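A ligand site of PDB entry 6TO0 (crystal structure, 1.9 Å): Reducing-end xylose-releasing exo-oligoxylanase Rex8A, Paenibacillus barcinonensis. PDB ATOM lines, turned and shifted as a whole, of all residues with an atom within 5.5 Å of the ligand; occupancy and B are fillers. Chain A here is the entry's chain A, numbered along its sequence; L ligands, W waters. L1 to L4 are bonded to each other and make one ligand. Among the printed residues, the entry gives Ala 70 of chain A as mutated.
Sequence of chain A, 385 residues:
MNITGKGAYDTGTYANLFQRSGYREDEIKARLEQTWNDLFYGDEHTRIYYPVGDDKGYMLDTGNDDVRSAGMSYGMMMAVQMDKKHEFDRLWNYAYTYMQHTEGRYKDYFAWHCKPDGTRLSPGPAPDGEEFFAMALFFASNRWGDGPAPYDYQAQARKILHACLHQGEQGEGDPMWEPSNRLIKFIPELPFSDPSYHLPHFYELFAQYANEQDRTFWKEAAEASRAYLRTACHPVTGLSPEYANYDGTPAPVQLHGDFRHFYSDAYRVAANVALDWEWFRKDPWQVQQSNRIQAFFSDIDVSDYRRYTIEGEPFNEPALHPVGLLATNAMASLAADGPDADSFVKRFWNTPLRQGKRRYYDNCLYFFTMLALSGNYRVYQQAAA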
ATOM      1  N   ASP A  61      29.777 -29.529  -5.006  1.00  0.00           N
ATOM      2  CA  ASP A  61      29.803 -28.660  -3.819  1.00  0.00           C
ATOM      3  C   ASP A  61      29.285 -29.518  -2.666  1.00  0.00           C
ATOM      4  O   ASP A  61      28.065 -29.635  -2.496  1.00  0.00           O
ATOM      5  CB  ASP A  61      29.033 -27.352  -3.975  1.00  0.00           C
ATOM      6  CG  ASP A  61      29.210 -26.469  -2.749  1.00  0.00           C
ATOM      7  OD1 ASP A  61      29.600 -27.010  -1.687  1.00  0.00           O
ATOM      8  OD2 ASP A  61      28.936 -25.267  -2.856  1.00  0.00           O
ATOM      9  N   ASN A  64      26.825 -28.072  -0.035  1.00  0.00           N
ATOM     10  CA  ASN A  64      25.467 -27.670  -0.455  1.00  0.00           C
ATOM     11  C   ASN A  64      24.768 -28.797  -1.214  1.00  0.00           C
ATOM     12  O   ASN A  64      23.635 -28.580  -1.655  1.00  0.00           O
ATOM     13  CB  ASN A  64      25.557 -26.401  -1.289  1.00  0.00           C
ATOM     14  CG  ASN A  64      25.966 -25.206  -0.437  1.00  0.00           C
ATOM     15  OD1 ASN A  64      25.241 -24.834   0.471  1.00  0.00           O
ATOM     16  ND2 ASN A  64      27.126 -24.630  -0.720  1.00  0.00           N
ATOM     17  N   ARG A  68      27.691 -26.757  -9.178  1.00  0.00           N
ATOM     18  CA  ARG A  68      27.641 -25.292  -9.432  1.00  0.00           C
ATOM     19  C   ARG A  68      28.436 -24.979 -10.703  1.00  0.00           C
ATOM     20  O   ARG A  68      29.454 -25.640 -10.926  1.00  0.00           O
ATOM     21  CB  ARG A  68      28.177 -24.568  -8.199  1.00  0.00           C
ATOM     22  CG  ARG A  68      27.207 -24.681  -7.030  1.00  0.00           C
ATOM     23  CD  ARG A  68      27.642 -24.148  -5.690  1.00  0.00           C
ATOM     24  NE  ARG A  68      26.496 -24.317  -4.817  1.00  0.00           N
ATOM     25  CZ  ARG A  68      26.036 -23.458  -3.931  1.00  0.00           C
ATOM     26  NH1 ARG A  68      26.671 -22.317  -3.684  1.00  0.00           N
ATOM     27  NH2 ARG A  68      24.940 -23.754  -3.254  1.00  0.00           N
ATOM     28  N   SER A  69      27.978 -24.014 -11.495  1.00  0.00           N
ATOM     29  CA  SER A  69      28.671 -23.577 -12.733  1.00  0.00           C
ATOM     30  C   SER A  69      30.100 -23.114 -12.392  1.00  0.00           C
ATOM     31  O   SER A  69      31.022 -23.471 -13.119  1.00  0.00           O
ATOM     32  CB  SER A  69      27.900 -22.557 -13.499  1.00  0.00           C
ATOM     33  OG  SER A  69      27.716 -21.366 -12.751  1.00  0.00           O
ATOM     34  N   ALA A  70      30.289 -22.436 -11.258  1.00  0.00           N
ATOM     35  CA  ALA A  70      31.636 -22.007 -10.802  1.00  0.00           C
ATOM     36  C   ALA A  70      32.512 -23.259 -10.629  1.00  0.00           C
ATOM     37  O   ALA A  70      33.642 -23.269 -11.153  1.00  0.00           O
ATOM     38  CB  ALA A  70      31.521 -21.199  -9.536  1.00  0.00           C
ATOM     39  N   TYR A  74      35.776 -24.313 -12.751  1.00  0.00           N
ATOM     40  CA  TYR A  74      37.049 -24.497 -12.004  1.00  0.00           C
ATOM     41  C   TYR A  74      37.683 -25.837 -12.389  1.00  0.00           C
ATOM     42  O   TYR A  74      38.903 -25.883 -12.667  1.00  0.00           O
ATOM     43  CB  TYR A  74      36.855 -24.519 -10.490  1.00  0.00           C
ATOM     44  CG  TYR A  74      36.465 -23.220  -9.832  1.00  0.00           C
ATOM     45  CD1 TYR A  74      36.632 -21.993 -10.444  1.00  0.00           C
ATOM     46  CD2 TYR A  74      35.918 -23.238  -8.554  1.00  0.00           C
ATOM     47  CE1 TYR A  74      36.271 -20.807  -9.798  1.00  0.00           C
ATOM     48  CE2 TYR A  74      35.527 -22.083  -7.908  1.00  0.00           C
ATOM     49  CZ  TYR A  74      35.709 -20.858  -8.528  1.00  0.00           C
ATOM     50  OH  TYR A  74      35.343 -19.736  -7.842  1.00  0.00           O
ATOM     51  N   TRP A 112      23.001 -21.886 -12.892  1.00  0.00           N
ATOM     52  CA  TRP A 112      24.167 -21.777 -11.964  1.00  0.00           C
ATOM     53  C   TRP A 112      24.326 -23.026 -11.104  1.00  0.00           C
ATOM     54  O   TRP A 112      25.445 -23.253 -10.626  1.00  0.00           O
ATOM     55  CB  TRP A 112      24.096 -20.490 -11.139  1.00  0.00           C
ATOM     56  CG  TRP A 112      23.201 -20.506  -9.942  1.00  0.00           C
ATOM     57  CD1 TRP A 112      21.893 -20.127  -9.864  1.00  0.00           C
ATOM     58  CD2 TRP A 112      23.596 -20.852  -8.602  1.00  0.00           C
ATOM     59  NE1 TRP A 112      21.456 -20.193  -8.564  1.00  0.00           N
ATOM     60  CE2 TRP A 112      22.462 -20.663  -7.774  1.00  0.00           C
ATOM     61  CE3 TRP A 112      24.795 -21.282  -8.029  1.00  0.00           C
ATOM     62  CZ2 TRP A 112      22.498 -20.923  -6.402  1.00  0.00           C
ATOM     63  CZ3 TRP A 112      24.820 -21.535  -6.678  1.00  0.00           C
ATOM     64  CH2 TRP A 112      23.698 -21.339  -5.867  1.00  0.00           C
ATOM     65  N   GLY A 124      18.854 -19.145 -13.239  1.00  0.00           N
ATOM     66  CA  GLY A 124      19.729 -17.964 -13.293  1.00  0.00           C
ATOM     67  C   GLY A 124      21.201 -18.351 -13.456  1.00  0.00           C
ATOM     68  O   GLY A 124      21.631 -19.384 -12.936  1.00  0.00           O
ATOM     69  N   PRO A 125      22.004 -17.586 -14.224  1.00  0.00           N
ATOM     70  CA  PRO A 125      23.425 -17.877 -14.341  1.00  0.00           C
ATOM     71  C   PRO A 125      24.301 -17.098 -13.358  1.00  0.00           C
ATOM     72  O   PRO A 125      23.848 -16.126 -12.762  1.00  0.00           O
ATOM     73  CB  PRO A 125      23.684 -17.419 -15.785  1.00  0.00           C
ATOM     74  CG  PRO A 125      22.864 -16.158 -15.875  1.00  0.00           C
ATOM     75  CD  PRO A 125      21.587 -16.493 -15.113  1.00  0.00           C
ATOM     76  N   ALA A 126      25.532 -17.573 -13.198  1.00  0.00           N
ATOM     77  CA  ALA A 126      26.591 -16.979 -12.356  1.00  0.00           C
ATOM     78  C   ALA A 126      27.730 -16.549 -13.282  1.00  0.00           C
ATOM     79  O   ALA A 126      28.370 -17.408 -13.890  1.00  0.00           O
ATOM     80  CB  ALA A 126      27.017 -17.975 -11.328  1.00  0.00           C
ATOM     81  N   ASP A 128      30.707 -15.648 -12.973  1.00  0.00           N
ATOM     82  CA  ASP A 128      32.045 -16.181 -12.618  1.00  0.00           C
ATOM     83  C   ASP A 128      32.209 -17.558 -13.255  1.00  0.00           C
ATOM     84  O   ASP A 128      33.343 -17.910 -13.605  1.00  0.00           O
ATOM     85  CB  ASP A 128      32.300 -16.122 -11.106  1.00  0.00           C
ATOM     86  CG  ASP A 128      31.361 -16.946 -10.237  1.00  0.00           C
ATOM     87  OD1 ASP A 128      30.148 -16.957 -10.522  1.00  0.00           O
ATOM     88  OD2 ASP A 128      31.875 -17.534  -9.253  1.00  0.00           O
ATOM     89  N   GLY A 129      31.114 -18.299 -13.438  1.00  0.00           N
ATOM     90  CA  GLY A 129      31.130 -19.591 -14.139  1.00  0.00           C
ATOM     91  C   GLY A 129      31.407 -19.372 -15.618  1.00  0.00           C
ATOM     92  O   GLY A 129      32.359 -19.957 -16.139  1.00  0.00           O
ATOM     93  N   PHE A 186      27.279  -9.007 -10.780  1.00  0.00           N
ATOM     94  CA  PHE A 186      26.943 -10.141  -9.906  1.00  0.00           C
ATOM     95  C   PHE A 186      25.978 -11.097 -10.633  1.00  0.00           C
ATOM     96  O   PHE A 186      26.211 -12.298 -10.646  1.00  0.00           O
ATOM     97  CB  PHE A 186      26.343  -9.643  -8.587  1.00  0.00           C
ATOM     98  CG  PHE A 186      25.663 -10.736  -7.808  1.00  0.00           C
ATOM     99  CD1 PHE A 186      26.367 -11.870  -7.420  1.00  0.00           C
ATOM    100  CD2 PHE A 186      24.330 -10.636  -7.470  1.00  0.00           C
ATOM    101  CE1 PHE A 186      25.738 -12.878  -6.711  1.00  0.00           C
ATOM    102  CE2 PHE A 186      23.699 -11.646  -6.751  1.00  0.00           C
ATOM    103  CZ  PHE A 186      24.408 -12.764  -6.370  1.00  0.00           C
ATOM    104  N   ILE A 187      24.883 -10.564 -11.162  1.00  0.00           N
ATOM    105  CA  ILE A 187      23.947 -11.340 -12.020  1.00  0.00           C
ATOM    106  C   ILE A 187      23.431 -10.390 -13.102  1.00  0.00           C
ATOM    107  O   ILE A 187      23.506  -9.171 -12.961  1.00  0.00           O
ATOM    108  CB  ILE A 187      22.787 -11.983 -11.224  1.00  0.00           C
ATOM    109  CG1 ILE A 187      21.901 -10.955 -10.520  1.00  0.00           C
ATOM    110  CG2 ILE A 187      23.293 -13.044 -10.243  1.00  0.00           C
ATOM    111  CD1 ILE A 187      20.580 -11.549 -10.010  1.00  0.00           C
ATOM    112  N   TYR A 197      34.805 -11.723  -8.937  1.00  0.00           N
ATOM    113  CA  TYR A 197      34.460 -12.086 -10.338  1.00  0.00           C
ATOM    114  C   TYR A 197      35.387 -11.361 -11.327  1.00  0.00           C
ATOM    115  O   TYR A 197      35.363 -11.725 -12.517  1.00  0.00           O
ATOM    116  CB  TYR A 197      33.015 -11.731 -10.688  1.00  0.00           C
ATOM    117  CG  TYR A 197      31.944 -12.551 -10.016  1.00  0.00           C
ATOM    118  CD1 TYR A 197      32.195 -13.365  -8.918  1.00  0.00           C
ATOM    119  CD2 TYR A 197      30.636 -12.463 -10.456  1.00  0.00           C
ATOM    120  CE1 TYR A 197      31.196 -14.087  -8.301  1.00  0.00           C
ATOM    121  CE2 TYR A 197      29.617 -13.185  -9.852  1.00  0.00           C
ATOM    122  CZ  TYR A 197      29.892 -13.995  -8.760  1.00  0.00           C
ATOM    123  OH  TYR A 197      28.888 -14.695  -8.171  1.00  0.00           O
ATOM    124  N   TYR A 243      30.054  -8.568  -2.106  1.00  0.00           N
ATOM    125  CA  TYR A 243      29.295  -7.781  -3.121  1.00  0.00           C
ATOM    126  C   TYR A 243      29.648  -6.306  -2.995  1.00  0.00           C
ATOM    127  O   TYR A 243      29.673  -5.771  -1.860  1.00  0.00           O
ATOM    128  CB  TYR A 243      27.774  -7.927  -3.029  1.00  0.00           C
ATOM    129  CG  TYR A 243      27.159  -9.300  -3.155  1.00  0.00           C
ATOM    130  CD1 TYR A 243      27.868 -10.421  -3.575  1.00  0.00           C
ATOM    131  CD2 TYR A 243      25.821  -9.477  -2.861  1.00  0.00           C
ATOM    132  CE1 TYR A 243      27.262 -11.670  -3.670  1.00  0.00           C
ATOM    133  CE2 TYR A 243      25.197 -10.713  -2.966  1.00  0.00           C
ATOM    134  CZ  TYR A 243      25.928 -11.821  -3.361  1.00  0.00           C
ATOM    135  OH  TYR A 243      25.310 -13.043  -3.433  1.00  0.00           O
ATOM    136  N   HIS A 256      18.875 -12.251   0.510  1.00  0.00           N
ATOM    137  CA  HIS A 256      19.479 -13.590   0.766  1.00  0.00           C
ATOM    138  C   HIS A 256      20.738 -13.489   1.648  1.00  0.00           C
ATOM    139  O   HIS A 256      21.336 -14.530   1.888  1.00  0.00           O
ATOM    140  CB  HIS A 256      19.732 -14.340  -0.560  1.00  0.00           C
ATOM    141  CG  HIS A 256      20.806 -13.763  -1.423  1.00  0.00           C
ATOM    142  ND1 HIS A 256      20.606 -12.652  -2.209  1.00  0.00           N
ATOM    143  CD2 HIS A 256      22.095 -14.138  -1.616  1.00  0.00           C
ATOM    144  CE1 HIS A 256      21.725 -12.354  -2.840  1.00  0.00           C
ATOM    145  NE2 HIS A 256      22.662 -13.248  -2.488  1.00  0.00           N
ATOM    146  N   PHE A 259      26.435  -9.296   2.399  1.00  0.00           N
ATOM    147  CA  PHE A 259      27.673  -9.610   1.621  1.00  0.00           C
ATOM    148  C   PHE A 259      28.658  -8.446   1.696  1.00  0.00           C
ATOM    149  O   PHE A 259      29.534  -8.311   0.822  1.00  0.00           O
ATOM    150  CB  PHE A 259      27.269 -10.012   0.214  1.00  0.00           C
ATOM    151  CG  PHE A 259      26.551 -11.337   0.171  1.00  0.00           C
ATOM    152  CD1 PHE A 259      27.268 -12.525   0.059  1.00  0.00           C
ATOM    153  CD2 PHE A 259      25.178 -11.408   0.259  1.00  0.00           C
ATOM    154  CE1 PHE A 259      26.608 -13.752   0.020  1.00  0.00           C
ATOM    155  CE2 PHE A 259      24.524 -12.632   0.232  1.00  0.00           C
ATOM    156  CZ  PHE A 259      25.232 -13.802   0.112  1.00  0.00           C
ATOM    157  N   SER A 264      33.827 -15.796   2.191  1.00  0.00           N
ATOM    158  CA  SER A 264      34.145 -16.803   1.145  1.00  0.00           C
ATOM    159  C   SER A 264      34.439 -16.180  -0.237  1.00  0.00           C
ATOM    160  O   SER A 264      35.543 -16.437  -0.753  1.00  0.00           O
ATOM    161  CB  SER A 264      33.051 -17.834   1.061  1.00  0.00           C
ATOM    162  OG  SER A 264      32.775 -18.369   2.347  1.00  0.00           O
ATOM    163  N   ASP A 265      33.499 -15.480  -0.877  1.00  0.00           N
ATOM    164  CA  ASP A 265      33.689 -15.010  -2.280  1.00  0.00           C
ATOM    165  C   ASP A 265      34.987 -14.196  -2.380  1.00  0.00           C
ATOM    166  O   ASP A 265      35.790 -14.430  -3.324  1.00  0.00           O
ATOM    167  CB  ASP A 265      32.561 -14.104  -2.767  1.00  0.00           C
ATOM    168  CG  ASP A 265      31.299 -14.826  -3.192  1.00  0.00           C
ATOM    169  OD1 ASP A 265      31.083 -15.983  -2.742  1.00  0.00           O
ATOM    170  OD2 ASP A 265      30.542 -14.227  -3.990  1.00  0.00           O
ATOM    171  N   ARG A 268      39.055 -14.927  -3.203  1.00  0.00           N
ATOM    172  CA  ARG A 268      39.677 -15.085  -4.557  1.00  0.00           C
ATOM    173  C   ARG A 268      40.318 -13.789  -5.054  1.00  0.00           C
ATOM    174  O   ARG A 268      41.182 -13.866  -5.922  1.00  0.00           O
ATOM    175  CB  ARG A 268      38.660 -15.645  -5.540  1.00  0.00           C
ATOM    176  CG  ARG A 268      38.128 -16.999  -5.083  1.00  0.00           C
ATOM    177  CD  ARG A 268      37.391 -17.791  -6.136  1.00  0.00           C
ATOM    178  NE  ARG A 268      36.473 -16.998  -6.942  1.00  0.00           N
ATOM    179  CZ  ARG A 268      35.209 -16.696  -6.622  1.00  0.00           C
ATOM    180  NH1 ARG A 268      34.682 -17.102  -5.483  1.00  0.00           N
ATOM    181  NH2 ARG A 268      34.475 -15.983  -7.461  1.00  0.00           N
ATOM    182  N   LEU A 320      34.163 -19.867   7.202  1.00  0.00           N
ATOM    183  CA  LEU A 320      33.638 -21.192   6.771  1.00  0.00           C
ATOM    184  C   LEU A 320      34.761 -21.980   6.063  1.00  0.00           C
ATOM    185  O   LEU A 320      34.825 -23.205   6.233  1.00  0.00           O
ATOM    186  CB  LEU A 320      32.418 -20.991   5.881  1.00  0.00           C
ATOM    187  CG  LEU A 320      31.875 -22.234   5.183  1.00  0.00           C
ATOM    188  CD1 LEU A 320      31.505 -23.311   6.183  1.00  0.00           C
ATOM    189  CD2 LEU A 320      30.673 -21.878   4.310  1.00  0.00           C
ATOM    190  N   HIS A 321      35.611 -21.303   5.290  1.00  0.00           N
ATOM    191  CA  HIS A 321      36.621 -21.943   4.421  1.00  0.00           C
ATOM    192  C   HIS A 321      38.002 -21.404   4.756  1.00  0.00           C
ATOM    193  O   HIS A 321      38.584 -20.674   3.944  1.00  0.00           O
ATOM    194  CB  HIS A 321      36.251 -21.709   2.945  1.00  0.00           C
ATOM    195  CG  HIS A 321      34.939 -22.272   2.547  1.00  0.00           C
ATOM    196  ND1 HIS A 321      34.667 -23.628   2.556  1.00  0.00           N
ATOM    197  CD2 HIS A 321      33.811 -21.668   2.106  1.00  0.00           C
ATOM    198  CE1 HIS A 321      33.429 -23.831   2.155  1.00  0.00           C
ATOM    199  NE2 HIS A 321      32.884 -22.644   1.865  1.00  0.00           N
ATOM    200  N   TYR A 360      34.824 -28.539  -0.379  1.00  0.00           N
ATOM    201  CA  TYR A 360      34.832 -28.234  -1.840  1.00  0.00           C
ATOM    202  C   TYR A 360      35.506 -26.878  -2.107  1.00  0.00           C
ATOM    203  O   TYR A 360      36.483 -26.824  -2.894  1.00  0.00           O
ATOM    204  CB  TYR A 360      33.406 -28.291  -2.395  1.00  0.00           C
ATOM    205  CG  TYR A 360      33.123 -27.458  -3.598  1.00  0.00           C
ATOM    206  CD1 TYR A 360      33.357 -27.911  -4.891  1.00  0.00           C
ATOM    207  CD2 TYR A 360      32.507 -26.216  -3.450  1.00  0.00           C
ATOM    208  CE1 TYR A 360      33.023 -27.139  -5.989  1.00  0.00           C
ATOM    209  CE2 TYR A 360      32.158 -25.443  -4.541  1.00  0.00           C
ATOM    210  CZ  TYR A 360      32.416 -25.905  -5.810  1.00  0.00           C
ATOM    211  OH  TYR A 360      32.083 -25.098  -6.862  1.00  0.00           O
ATOM    212  N   TYR A 361      35.027 -25.805  -1.479  1.00  0.00           N
ATOM    213  CA  TYR A 361      35.501 -24.446  -1.832  1.00  0.00           C
ATOM    214  C   TYR A 361      36.960 -24.290  -1.410  1.00  0.00           C
ATOM    215  O   TYR A 361      37.752 -23.758  -2.206  1.00  0.00           O
ATOM    216  CB  TYR A 361      34.595 -23.378  -1.238  1.00  0.00           C
ATOM    217  CG  TYR A 361      34.885 -21.978  -1.730  1.00  0.00           C
ATOM    218  CD1 TYR A 361      34.586 -21.608  -3.028  1.00  0.00           C
ATOM    219  CD2 TYR A 361      35.437 -21.036  -0.891  1.00  0.00           C
ATOM    220  CE1 TYR A 361      34.860 -20.328  -3.490  1.00  0.00           C
ATOM    221  CE2 TYR A 361      35.695 -19.744  -1.323  1.00  0.00           C
ATOM    222  CZ  TYR A 361      35.383 -19.394  -2.617  1.00  0.00           C
ATOM    223  OH  TYR A 361      35.637 -18.117  -3.041  1.00  0.00           O
HETATM  224  O1  LIG L   1      30.800 -21.638   0.477  1.00  0.00           O
HETATM  225  C1  LIG L   1      31.168 -21.330  -0.828  1.00  0.00           C
HETATM  226  C2  LIG L   1      30.292 -22.185  -1.719  1.00  0.00           C
HETATM  227  C3  LIG L   1      30.547 -21.827  -3.139  1.00  0.00           C
HETATM  228  C4  LIG L   1      30.162 -20.371  -3.308  1.00  0.00           C
HETATM  229  C5  LIG L   1      31.110 -19.539  -2.448  1.00  0.00           C
HETATM  230  O2  LIG L   1      30.692 -23.558  -1.576  1.00  0.00           O
HETATM  231  O3  LIG L   1      29.682 -22.667  -3.923  1.00  0.00           O
HETATM  232  O4  LIG L   1      30.378 -20.053  -4.669  1.00  0.00           O
HETATM  233  O5  LIG L   1      30.880 -19.928  -1.050  1.00  0.00           O
HETATM  234  C1  LG2 L   2      29.395 -19.169  -5.226  1.00  0.00           C
HETATM  235  C2  LG2 L   2      29.615 -19.072  -6.703  1.00  0.00           C
HETATM  236  C3  LG2 L   2      28.586 -18.179  -7.338  1.00  0.00           C
HETATM  237  C4  LG2 L   2      27.184 -18.490  -6.850  1.00  0.00           C
HETATM  238  C5  LG2 L   2      27.175 -18.773  -5.345  1.00  0.00           C
HETATM  239  O1  LG2 L   2      30.933 -18.503  -6.919  1.00  0.00           O
HETATM  240  O2  LG2 L   2      28.690 -18.436  -8.757  1.00  0.00           O
HETATM  241  O3  LG2 L   2      26.359 -17.317  -6.934  1.00  0.00           O
HETATM  242  O4  LG2 L   2      28.124 -19.789  -5.061  1.00  0.00           O
HETATM  243  C1  LG3 L   3      24.986 -17.536  -7.341  1.00  0.00           C
HETATM  244  C2  LG3 L   3      24.110 -16.773  -6.451  1.00  0.00           C
HETATM  245  C3  LG3 L   3      22.704 -16.766  -7.053  1.00  0.00           C
HETATM  246  C4  LG3 L   3      22.749 -16.188  -8.445  1.00  0.00           C
HETATM  247  C5  LG3 L   3      23.633 -17.020  -9.293  1.00  0.00           C
HETATM  248  O1  LG3 L   3      24.125 -17.546  -5.172  1.00  0.00           O
HETATM  249  O2  LG3 L   3      21.939 -15.862  -6.317  1.00  0.00           O
HETATM  250  O3  LG3 L   3      21.441 -16.249  -9.021  1.00  0.00           O
HETATM  251  O4  LG3 L   3      24.967 -16.990  -8.697  1.00  0.00           O
HETATM  252  O1  LG4 L   4      23.785 -21.011  -1.888  1.00  0.00           O
HETATM  253  C1  LG4 L   4      24.684 -19.847  -2.033  1.00  0.00           C
HETATM  254  C2  LG4 L   4      24.107 -18.847  -2.964  1.00  0.00           C
HETATM  255  O2  LG4 L   4      24.664 -17.503  -3.048  1.00  0.00           O
HETATM  256  C3  LG4 L   4      22.867 -18.264  -2.370  1.00  0.00           C
HETATM  257  O3  LG4 L   4      22.092 -19.379  -1.991  1.00  0.00           O
HETATM  258  C4  LG4 L   4      22.434 -17.683  -3.639  1.00  0.00           C
HETATM  259  O4  LG4 L   4      21.418 -16.771  -3.345  1.00  0.00           O
HETATM  260  C5  LG4 L   4      23.721 -16.972  -4.033  1.00  0.00           C
HETATM  261  O   HOH W   1      30.206 -19.105   1.990  1.00  0.00           O
HETATM  262  O   HOH W   2      28.509 -22.737   1.171  1.00  0.00           O
HETATM  263  O   HOH W   3      28.721 -15.238  -5.481  1.00  0.00           O
HETATM  264  O   HOH W   4      32.799 -20.583  -6.250  1.00  0.00           O
HETATM  265  O   HOH W   5      21.436 -15.630 -11.667  1.00  0.00           O
HETATM  266  O   HOH W   6      31.199 -22.773  -6.428  1.00  0.00           O
HETATM  267  O   HOH W   7      26.689 -14.795  -9.596  1.00  0.00           O
HETATM  268  O   HOH W   8      26.709 -15.269  -3.792  1.00  0.00           O
HETATM  269  O   HOH W   9      27.959 -21.031  -9.935  1.00  0.00           O
HETATM  270  O   HOH W  10      19.341 -18.008  -8.489  1.00  0.00           O
HETATM  271  O   HOH W  11      24.620 -22.221   0.738  1.00  0.00           O
HETATM  272  O   HOH W  12      32.144 -16.575  -5.422  1.00  0.00           O
HETATM  273  O   HOH W  13      19.795 -14.125  -7.210  1.00  0.00           O
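The side-chain carboxylate of Asp 61 sits at hydrogen-bond distance from an oxygen (O2) of LIG L1 (2.8 Å). The side-chain carboxylate (OD2) of Asp 128 is in hydrogen-bond range of an oxygen (O1) of LG2 L2 (2.7 Å). The guanidinium group (NH1) of Arg 68 sits at hydrogen-bond distance from an oxygen (O3) of LIG L1 (3.0 Å). A ring nitrogen (NE2) of His 321 is in hydrogen-bond range of an oxygen (O1) of LIG L1 (2.7 Å).
The guanidinium group of Arg 68 lies close to the side-chain amide nitrogen of Asn 64 (3.5 Å). The side-chain hydroxyl (OH) of Tyr 361 is in hydrogen-bond range of the guanidinium group (NH1) of Arg 268 (2.8 Å). OD1 of Asp 128 lies close to OH of Tyr 197. OH of Tyr 243 lies within hydrogen-bond range of NE2 of His 256 (2.8 Å). OD2 of Asp 61 sits at hydrogen-bond distance from ND2 of Asn 64 (2.9 Å). OD2 of Asp 61 lies within salt-bridge range of NE of Arg 68 (3.3 Å). O of Trp 112 sits at hydrogen-bond distance from N of Ser 69, 2.8 Å away. The guanidinium group (NH2) of Arg 268 lies within salt-bridge range of the side-chain carboxylate (OD2) of Asp 128.
Asn 64 touches the ligand. CB of Ala 70 touches O1 of LG2 L2, at 3.8 Å. CG of Trp 112 touches C5 of LG3 L3, at 3.6 Å. Pro 125 touches the ligand. Ala 126 touches the ligand. CZ of Phe 186 touches O2 of LG3 L3 (3.96 Å). CG2 of Ile 187 touches C4 of LG3 L3 (3.7 Å). OH of Tyr 197 touches C3 of LG2 L2 (3.6 Å). CD2 of His 256 touches O4 of LG4 L4, at 3.2 Å. Ser 264 touches the ligand. OD1 of Asp 265 touches C5 of LIG L1, at 3.6 Å. CD2 of Leu 320 touches O1 of LIG L1, at 3.8 Å. Tyr 360 touches the ligand. CG of Tyr 361 touches C1 of LIG L1, at 3.9 Å. Within 4 Å of the ligand: Asp 61, Asn 64, Arg 68, Ala 70, Trp 112, Pro 125, Ala 126, Asp 128, Phe 186, Ile 187, Tyr 197, His 256, Ser 264, Asp 265, Leu 320, His 321, Tyr 360 and Tyr 361.
Water W12 lies within hydrogen-bond range of the guanidinium group (NH1) of Arg 268, an oxygen (O1) of LG2 L2 and the side-chain carboxylate (OD1) of Asp 265. Water W10 bridges O3 of LG3 L3 and NE1 of Trp 112. Water W4 bridges O1 of LG2 L2 (2.9 Å) and OH of Tyr 74 (3.1 Å). Water W1 lies within hydrogen-bond range of OG of Ser 264 and O1 of LIG L1. Water W11 lies within hydrogen-bond range of OD1 of Asn 64 and O1 of LG4 L4. Water W3 lies within hydrogen-bond range of OD2 of Asp 265 (2.6 Å), OH of Tyr 197 (2.7 Å) and O3 of LG2 L2 (3.5 Å).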
